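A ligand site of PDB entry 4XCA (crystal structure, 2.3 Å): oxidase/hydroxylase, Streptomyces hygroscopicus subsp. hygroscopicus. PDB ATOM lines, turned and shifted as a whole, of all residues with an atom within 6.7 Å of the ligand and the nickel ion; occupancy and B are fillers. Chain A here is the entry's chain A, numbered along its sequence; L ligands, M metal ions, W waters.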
ATOM      1  N   ARG A  51       4.855  -5.466 -35.148  1.00  0.00           N
ATOM      2  CA  ARG A  51       5.072  -4.215 -35.860  1.00  0.00           C
ATOM      3  C   ARG A  51       4.416  -4.321 -37.242  1.00  0.00           C
ATOM      4  O   ARG A  51       4.407  -5.405 -37.814  1.00  0.00           O
ATOM      5  CB  ARG A  51       6.569  -3.945 -35.973  1.00  0.00           C
ATOM      6  CG  ARG A  51       6.968  -2.654 -36.676  1.00  0.00           C
ATOM      7  CD  ARG A  51       8.479  -2.621 -36.854  1.00  0.00           C
ATOM      8  NE  ARG A  51       8.960  -1.274 -37.161  1.00  0.00           N
ATOM      9  CZ  ARG A  51       9.191  -0.343 -36.237  1.00  0.00           C
ATOM     10  NH1 ARG A  51       8.991  -0.604 -34.952  1.00  0.00           N
ATOM     11  NH2 ARG A  51       9.624   0.861 -36.604  1.00  0.00           N
ATOM     12  N   TYR A  89       4.866   3.284 -39.764  1.00  0.00           N
ATOM     13  CA  TYR A  89       4.651   1.911 -39.290  1.00  0.00           C
ATOM     14  C   TYR A  89       3.587   1.895 -38.191  1.00  0.00           C
ATOM     15  O   TYR A  89       3.255   2.930 -37.617  1.00  0.00           O
ATOM     16  CB  TYR A  89       5.981   1.277 -38.796  1.00  0.00           C
ATOM     17  CG  TYR A  89       6.610   2.010 -37.639  1.00  0.00           C
ATOM     18  CD1 TYR A  89       7.535   3.037 -37.858  1.00  0.00           C
ATOM     19  CD2 TYR A  89       6.276   1.705 -36.328  1.00  0.00           C
ATOM     20  CE1 TYR A  89       8.094   3.726 -36.794  1.00  0.00           C
ATOM     21  CE2 TYR A  89       6.833   2.392 -35.249  1.00  0.00           C
ATOM     22  CZ  TYR A  89       7.744   3.397 -35.500  1.00  0.00           C
ATOM     23  OH  TYR A  89       8.304   4.074 -34.444  1.00  0.00           O
ATOM     24  N   LEU A  91       2.142  -0.075 -34.532  1.00  0.00           N
ATOM     25  CA  LEU A  91       2.569  -0.865 -33.375  1.00  0.00           C
ATOM     26  C   LEU A  91       1.343  -1.399 -32.637  1.00  0.00           C
ATOM     27  O   LEU A  91       0.482  -0.625 -32.212  1.00  0.00           O
ATOM     28  CB  LEU A  91       3.427  -0.041 -32.407  1.00  0.00           C
ATOM     29  CG  LEU A  91       4.796   0.449 -32.861  1.00  0.00           C
ATOM     30  CD1 LEU A  91       5.432   1.326 -31.765  1.00  0.00           C
ATOM     31  CD2 LEU A  91       5.740  -0.712 -33.222  1.00  0.00           C
ATOM     32  N   ARG A  93       0.578  -3.648 -29.246  1.00  0.00           N
ATOM     33  CA  ARG A  93       1.211  -4.207 -28.056  1.00  0.00           C
ATOM     34  C   ARG A  93       0.215  -4.793 -27.065  1.00  0.00           C
ATOM     35  O   ARG A  93      -0.901  -4.297 -26.913  1.00  0.00           O
ATOM     36  CB  ARG A  93       2.067  -3.141 -27.373  1.00  0.00           C
ATOM     37  CG  ARG A  93       3.452  -3.018 -28.015  1.00  0.00           C
ATOM     38  CD  ARG A  93       4.306  -1.959 -27.360  1.00  0.00           C
ATOM     39  NE  ARG A  93       4.317  -2.094 -25.899  1.00  0.00           N
ATOM     40  CZ  ARG A  93       4.676  -1.114 -25.074  1.00  0.00           C
ATOM     41  NH1 ARG A  93       5.026   0.060 -25.556  1.00  0.00           N
ATOM     42  NH2 ARG A  93       4.655  -1.324 -23.758  1.00  0.00           N
ATOM     43  N   LEU A  99       9.083  -0.959 -23.809  1.00  0.00           N
ATOM     44  CA  LEU A  99       9.991  -0.329 -24.746  1.00  0.00           C
ATOM     45  C   LEU A  99      11.001   0.462 -23.943  1.00  0.00           C
ATOM     46  O   LEU A  99      10.661   1.456 -23.323  1.00  0.00           O
ATOM     47  CB  LEU A  99       9.241   0.570 -25.743  1.00  0.00           C
ATOM     48  CG  LEU A  99      10.043   1.224 -26.867  1.00  0.00           C
ATOM     49  CD1 LEU A  99      10.689   0.196 -27.786  1.00  0.00           C
ATOM     50  CD2 LEU A  99       9.129   2.097 -27.675  1.00  0.00           C
ATOM     51  N   HIS A 102      15.401   4.995 -25.507  1.00  0.00           N
ATOM     52  CA  HIS A 102      16.253   5.217 -26.668  1.00  0.00           C
ATOM     53  C   HIS A 102      16.198   6.705 -27.024  1.00  0.00           C
ATOM     54  O   HIS A 102      15.281   7.407 -26.598  1.00  0.00           O
ATOM     55  CB  HIS A 102      15.828   4.350 -27.846  1.00  0.00           C
ATOM     56  CG  HIS A 102      14.374   4.486 -28.207  1.00  0.00           C
ATOM     57  ND1 HIS A 102      13.359   3.989 -27.427  1.00  0.00           N
ATOM     58  CD2 HIS A 102      13.780   5.079 -29.267  1.00  0.00           C
ATOM     59  CE1 HIS A 102      12.195   4.271 -27.978  1.00  0.00           C
ATOM     60  NE2 HIS A 102      12.419   4.938 -29.102  1.00  0.00           N
ATOM     61  N   LYS A 137       8.855  12.691 -35.261  1.00  0.00           N
ATOM     62  CA  LYS A 137       7.931  11.592 -35.419  1.00  0.00           C
ATOM     63  C   LYS A 137       6.552  12.052 -34.958  1.00  0.00           C
ATOM     64  O   LYS A 137       6.433  12.721 -33.933  1.00  0.00           O
ATOM     65  CB  LYS A 137       8.423  10.382 -34.633  1.00  0.00           C
ATOM     66  CG  LYS A 137       7.790   9.098 -35.019  1.00  0.00           C
ATOM     67  CD  LYS A 137       8.533   7.930 -34.385  1.00  0.00           C
ATOM     68  CE  LYS A 137       9.804   7.641 -35.138  1.00  0.00           C
ATOM     69  NZ  LYS A 137      10.403   6.398 -34.610  1.00  0.00           N
ATOM     70  N   LEU A 139       3.251  10.456 -33.697  1.00  0.00           N
ATOM     71  CA  LEU A 139       2.611   9.254 -33.189  1.00  0.00           C
ATOM     72  C   LEU A 139       1.115   9.477 -33.099  1.00  0.00           C
ATOM     73  O   LEU A 139       0.652  10.350 -32.348  1.00  0.00           O
ATOM     74  CB  LEU A 139       3.157   8.875 -31.807  1.00  0.00           C
ATOM     75  CG  LEU A 139       4.674   8.739 -31.630  1.00  0.00           C
ATOM     76  CD1 LEU A 139       5.001   8.482 -30.157  1.00  0.00           C
ATOM     77  CD2 LEU A 139       5.228   7.619 -32.498  1.00  0.00           C
ATOM     78  N   TYR A 141      -2.051   7.912 -31.794  1.00  0.00           N
ATOM     79  CA  TYR A 141      -2.561   6.885 -30.910  1.00  0.00           C
ATOM     80  C   TYR A 141      -3.949   6.430 -31.338  1.00  0.00           C
ATOM     81  O   TYR A 141      -4.775   7.233 -31.766  1.00  0.00           O
ATOM     82  CB  TYR A 141      -2.551   7.393 -29.454  1.00  0.00           C
ATOM     83  CG  TYR A 141      -1.150   7.454 -28.923  1.00  0.00           C
ATOM     84  CD1 TYR A 141      -0.394   8.601 -29.044  1.00  0.00           C
ATOM     85  CD2 TYR A 141      -0.553   6.331 -28.358  1.00  0.00           C
ATOM     86  CE1 TYR A 141       0.907   8.650 -28.593  1.00  0.00           C
ATOM     87  CE2 TYR A 141       0.730   6.368 -27.904  1.00  0.00           C
ATOM     88  CZ  TYR A 141       1.457   7.536 -28.021  1.00  0.00           C
ATOM     89  OH  TYR A 141       2.745   7.593 -27.557  1.00  0.00           O
ATOM     90  N   ILE A 145      -4.397   5.619 -23.369  1.00  0.00           N
ATOM     91  CA  ILE A 145      -3.328   5.232 -22.482  1.00  0.00           C
ATOM     92  C   ILE A 145      -3.314   6.252 -21.369  1.00  0.00           C
ATOM     93  O   ILE A 145      -2.770   7.360 -21.518  1.00  0.00           O
ATOM     94  CB  ILE A 145      -1.973   5.164 -23.199  1.00  0.00           C
ATOM     95  CG1 ILE A 145      -2.080   4.262 -24.446  1.00  0.00           C
ATOM     96  CG2 ILE A 145      -0.893   4.646 -22.254  1.00  0.00           C
ATOM     97  CD1 ILE A 145      -0.852   4.285 -25.349  1.00  0.00           C
ATOM     98  N   GLY A 151       1.133   1.053 -20.140  1.00  0.00           N
ATOM     99  CA  GLY A 151       2.299   1.200 -20.993  1.00  0.00           C
ATOM    100  C   GLY A 151       2.456   2.616 -21.538  1.00  0.00           C
ATOM    101  O   GLY A 151       2.664   2.806 -22.740  1.00  0.00           O
ATOM    102  N   SER A 152       2.370   3.603 -20.665  1.00  0.00           N
ATOM    103  CA  SER A 152       2.425   4.995 -21.083  1.00  0.00           C
ATOM    104  C   SER A 152       3.805   5.411 -21.591  1.00  0.00           C
ATOM    105  O   SER A 152       4.823   5.056 -21.010  1.00  0.00           O
ATOM    106  CB  SER A 152       1.994   5.925 -19.944  1.00  0.00           C
ATOM    107  OG  SER A 152       2.853   5.817 -18.832  1.00  0.00           O
ATOM    108  N   PHE A 153       3.793   6.158 -22.681  1.00  0.00           N
ATOM    109  CA  PHE A 153       4.963   6.888 -23.156  1.00  0.00           C
ATOM    110  C   PHE A 153       5.596   7.616 -21.991  1.00  0.00           C
ATOM    111  O   PHE A 153       4.925   8.300 -21.221  1.00  0.00           O
ATOM    112  CB  PHE A 153       4.549   7.868 -24.240  1.00  0.00           C
ATOM    113  CG  PHE A 153       5.672   8.693 -24.772  1.00  0.00           C
ATOM    114  CD1 PHE A 153       6.074   9.861 -24.121  1.00  0.00           C
ATOM    115  CD2 PHE A 153       6.298   8.344 -25.956  1.00  0.00           C
ATOM    116  CE1 PHE A 153       7.094  10.634 -24.638  1.00  0.00           C
ATOM    117  CE2 PHE A 153       7.340   9.099 -26.470  1.00  0.00           C
ATOM    118  CZ  PHE A 153       7.731  10.251 -25.822  1.00  0.00           C
ATOM    119  N   CYS A 154       6.912   7.446 -21.847  1.00  0.00           N
ATOM    120  CA  CYS A 154       7.620   8.140 -20.803  1.00  0.00           C
ATOM    121  C   CYS A 154       8.911   8.687 -21.387  1.00  0.00           C
ATOM    122  O   CYS A 154       9.405   8.163 -22.388  1.00  0.00           O
ATOM    123  CB  CYS A 154       7.891   7.220 -19.607  1.00  0.00           C
ATOM    124  SG  CYS A 154       8.831   5.724 -19.978  1.00  0.00           S
ATOM    125  N   LEU A 198       1.082  12.666 -30.725  1.00  0.00           N
ATOM    126  CA  LEU A 198       2.255  13.056 -29.968  1.00  0.00           C
ATOM    127  C   LEU A 198       3.347  13.389 -30.991  1.00  0.00           C
ATOM    128  O   LEU A 198       3.898  12.507 -31.629  1.00  0.00           O
ATOM    129  CB  LEU A 198       2.677  11.965 -28.998  1.00  0.00           C
ATOM    130  CG  LEU A 198       3.671  12.308 -27.871  1.00  0.00           C
ATOM    131  CD1 LEU A 198       3.768  11.130 -26.905  1.00  0.00           C
ATOM    132  CD2 LEU A 198       5.068  12.687 -28.386  1.00  0.00           C
ATOM    133  N   LEU A 200       6.972  14.389 -31.814  1.00  0.00           N
ATOM    134  CA  LEU A 200       8.166  14.033 -31.049  1.00  0.00           C
ATOM    135  C   LEU A 200       9.472  14.422 -31.728  1.00  0.00           C
ATOM    136  O   LEU A 200       9.705  14.041 -32.866  1.00  0.00           O
ATOM    137  CB  LEU A 200       8.162  12.521 -30.804  1.00  0.00           C
ATOM    138  CG  LEU A 200       9.289  11.983 -29.939  1.00  0.00           C
ATOM    139  CD1 LEU A 200       9.258  12.723 -28.631  1.00  0.00           C
ATOM    140  CD2 LEU A 200       9.090  10.493 -29.722  1.00  0.00           C
ATOM    141  N   GLU A 202      12.950  13.415 -32.053  1.00  0.00           N
ATOM    142  CA  GLU A 202      13.570  12.125 -31.834  1.00  0.00           C
ATOM    143  C   GLU A 202      14.900  12.250 -31.087  1.00  0.00           C
ATOM    144  O   GLU A 202      15.505  11.243 -30.707  1.00  0.00           O
ATOM    145  CB  GLU A 202      13.774  11.386 -33.166  1.00  0.00           C
ATOM    146  CG  GLU A 202      12.482  10.740 -33.693  1.00  0.00           C
ATOM    147  CD  GLU A 202      12.024   9.566 -32.840  1.00  0.00           C
ATOM    148  OE1 GLU A 202      12.784   8.590 -32.707  1.00  0.00           O
ATOM    149  OE2 GLU A 202      10.899   9.597 -32.299  1.00  0.00           O
ATOM    150  N   LEU A 204      14.810  13.401 -28.196  1.00  0.00           N
ATOM    151  CA  LEU A 204      14.360  13.172 -26.832  1.00  0.00           C
ATOM    152  C   LEU A 204      14.625  11.720 -26.419  1.00  0.00           C
ATOM    153  O   LEU A 204      14.378  10.787 -27.203  1.00  0.00           O
ATOM    154  CB  LEU A 204      12.872  13.506 -26.690  1.00  0.00           C
ATOM    155  CG  LEU A 204      12.260  13.478 -25.286  1.00  0.00           C
ATOM    156  CD1 LEU A 204      12.632  14.712 -24.456  1.00  0.00           C
ATOM    157  CD2 LEU A 204      10.762  13.353 -25.414  1.00  0.00           C
ATOM    158  N   HIS A 206      13.406   8.623 -24.683  1.00  0.00           N
ATOM    159  CA  HIS A 206      12.012   8.245 -24.461  1.00  0.00           C
ATOM    160  C   HIS A 206      11.826   6.736 -24.608  1.00  0.00           C
ATOM    161  O   HIS A 206      12.704   6.036 -25.090  1.00  0.00           O
ATOM    162  CB  HIS A 206      11.097   8.975 -25.452  1.00  0.00           C
ATOM    163  CG  HIS A 206      11.330   8.570 -26.871  1.00  0.00           C
ATOM    164  ND1 HIS A 206      12.442   8.970 -27.586  1.00  0.00           N
ATOM    165  CD2 HIS A 206      10.631   7.753 -27.693  1.00  0.00           C
ATOM    166  CE1 HIS A 206      12.401   8.441 -28.797  1.00  0.00           C
ATOM    167  NE2 HIS A 206      11.311   7.706 -28.891  1.00  0.00           N
ATOM    168  N   GLY A 207      10.662   6.253 -24.194  1.00  0.00           N
ATOM    169  CA  GLY A 207      10.346   4.845 -24.225  1.00  0.00           C
ATOM    170  C   GLY A 207       8.914   4.734 -23.733  1.00  0.00           C
ATOM    171  O   GLY A 207       8.172   5.708 -23.784  1.00  0.00           O
ATOM    172  N   THR A 208       8.521   3.547 -23.272  1.00  0.00           N
ATOM    173  CA  THR A 208       7.225   3.404 -22.604  1.00  0.00           C
ATOM    174  C   THR A 208       7.385   2.532 -21.364  1.00  0.00           C
ATOM    175  O   THR A 208       8.323   1.724 -21.286  1.00  0.00           O
ATOM    176  CB  THR A 208       6.157   2.747 -23.499  1.00  0.00           C
ATOM    177  OG1 THR A 208       6.228   1.322 -23.351  1.00  0.00           O
ATOM    178  CG2 THR A 208       6.309   3.130 -24.984  1.00  0.00           C
ATOM    179  N   ARG A 217      -2.810  -2.279 -27.061  1.00  0.00           N
ATOM    180  CA  ARG A 217      -2.311  -0.913 -27.127  1.00  0.00           C
ATOM    181  C   ARG A 217      -1.893  -0.620 -28.578  1.00  0.00           C
ATOM    182  O   ARG A 217      -1.070  -1.356 -29.128  1.00  0.00           O
ATOM    183  CB  ARG A 217      -1.137  -0.740 -26.149  1.00  0.00           C
ATOM    184  CG  ARG A 217      -0.423   0.622 -26.176  1.00  0.00           C
ATOM    185  CD  ARG A 217       0.924   0.541 -25.476  1.00  0.00           C
ATOM    186  NE  ARG A 217       1.449   1.852 -25.141  1.00  0.00           N
ATOM    187  CZ  ARG A 217       2.118   2.639 -25.967  1.00  0.00           C
ATOM    188  NH1 ARG A 217       2.349   2.254 -27.213  1.00  0.00           N
ATOM    189  NH2 ARG A 217       2.558   3.824 -25.567  1.00  0.00           N
ATOM    190  N   LEU A 219      -0.951   2.111 -32.023  1.00  0.00           N
ATOM    191  CA  LEU A 219      -0.628   3.371 -32.661  1.00  0.00           C
ATOM    192  C   LEU A 219      -0.050   3.211 -34.069  1.00  0.00           C
ATOM    193  O   LEU A 219       0.374   2.131 -34.488  1.00  0.00           O
ATOM    194  CB  LEU A 219       0.342   4.190 -31.777  1.00  0.00           C
ATOM    195  CG  LEU A 219       1.771   3.724 -31.435  1.00  0.00           C
ATOM    196  CD1 LEU A 219       2.677   3.576 -32.649  1.00  0.00           C
ATOM    197  CD2 LEU A 219       2.423   4.719 -30.500  1.00  0.00           C
ATOM    198  N   ALA A 221       2.901   5.322 -36.400  1.00  0.00           N
ATOM    199  CA  ALA A 221       4.006   6.267 -36.275  1.00  0.00           C
ATOM    200  C   ALA A 221       4.508   6.682 -37.633  1.00  0.00           C
ATOM    201  O   ALA A 221       4.755   5.839 -38.500  1.00  0.00           O
ATOM    202  CB  ALA A 221       5.138   5.647 -35.466  1.00  0.00           C
HETATM  203  C1  LIG L   1       8.745   4.225 -31.256  1.00  0.00           C
HETATM  204  O1  LIG L   1       9.926   4.482 -31.597  1.00  0.00           O
HETATM  205  O2  LIG L   1       8.046   3.447 -31.946  1.00  0.00           O
HETATM  206  C2  LIG L   1       8.161   4.848 -30.018  1.00  0.00           C
HETATM  207  O3  LIG L   1       8.738   5.765 -29.458  1.00  0.00           O
HETATM  208  C3  LIG L   1       6.850   4.315 -29.493  1.00  0.00           C
HETATM  209  C4  LIG L   1       6.265   5.282 -28.489  1.00  0.00           C
HETATM  210  C5  LIG L   1       5.014   4.658 -27.912  1.00  0.00           C
HETATM  211  O4  LIG L   1       4.229   5.366 -27.229  1.00  0.00           O
HETATM  212  O5  LIG L   1       4.749   3.427 -28.088  1.00  0.00           O
HETATM  213 NI    NI M   1      10.834   6.054 -30.175  1.00  0.00          NI
HETATM  214  O   HOH W   1       9.924   7.606 -31.208  1.00  0.00           O
HETATM  215  O   HOH W   2      12.269   6.669 -31.241  1.00  0.00           O
HETATM  216  O   HOH W   3      13.078   4.297 -33.040  1.00  0.00           O
HETATM  217  O   HOH W   4       5.453   0.729 -28.355  1.00  0.00           O
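The nearest printed residue that does not touch the nickel ion is Glu 202 (4.1 Å).
OH of Tyr 89 lies within hydrogen-bond range of NZ of Lys 137 (3.1 Å). O of Tyr 89 lies within hydrogen-bond range of N of Ala 221, at 2.7 Å. N of Arg 217 sits at hydrogen-bond distance from O of Arg 93, at 2.8 Å. The backbone NH (N) of Thr 208 lies within hydrogen-bond range of the backbone carbonyl oxygen (O) of Leu 99, at 3.0 Å. The guanidinium group (NH1) of Arg 93 sits at hydrogen-bond distance from the side-chain hydroxyl (OG1) of Thr 208 (2.8 Å). The side-chain carboxylate (OE1) of Glu 202 lies within salt-bridge range of the side-chain amino group (NZ) of Lys 137, 3.8 Å away. The backbone carbonyl oxygen of Lys 137 lies within hydrogen-bond range of the backbone NH of Leu 200, 2.8 Å away. O of Leu 139 sits at hydrogen-bond distance from N of Leu 198, 2.9 Å away.
Water W4 lies within hydrogen-bond range of an oxygen (O5) of the ligand (2.8 Å) and the guanidinium group of Arg 93 (2.9 Å).
The side-chain hydroxyl of Tyr 89 is in hydrogen-bond range of an oxygen (O2) of the ligand. O4 of the ligand sits at hydrogen-bond distance from OH of Tyr 141 (2.7 Å). The guanidinium group of Arg 217 lies within salt-bridge range of an oxygen (O5) of the ligand, 2.8 Å away. The side-chain amino group of Lys 137 lies close to an oxygen (O1) of the ligand (3.6 Å).
Leu 91 touches the ligand (CD1 to O2, 3.4 Å). CD2 of Leu 99 touches C3 of the ligand, 3.7 Å away. CD1 of Leu 139 touches C4 of the ligand (3.8 Å). CD2 of Phe 153 touches O4 of the ligand, at 3.8 Å. Thr 208 touches the ligand (CG2 to O5, 3.5 Å). Leu 219 touches the ligand (CD2 to O5, 3.6 Å). Hydrophobic or aromatic side chains that line the ligand: Tyr 89, Leu 91, Leu 99, Leu 139, Tyr 141, Phe 153, His 206 and Leu 219. The nearest printed residue that does not touch the ligand is Arg 93 (4.2 Å).
The nickel ion is bound by water W2, water W1, NE2 of His 206, NE2 of His 102, O3 of the ligand and O1 of the ligand.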
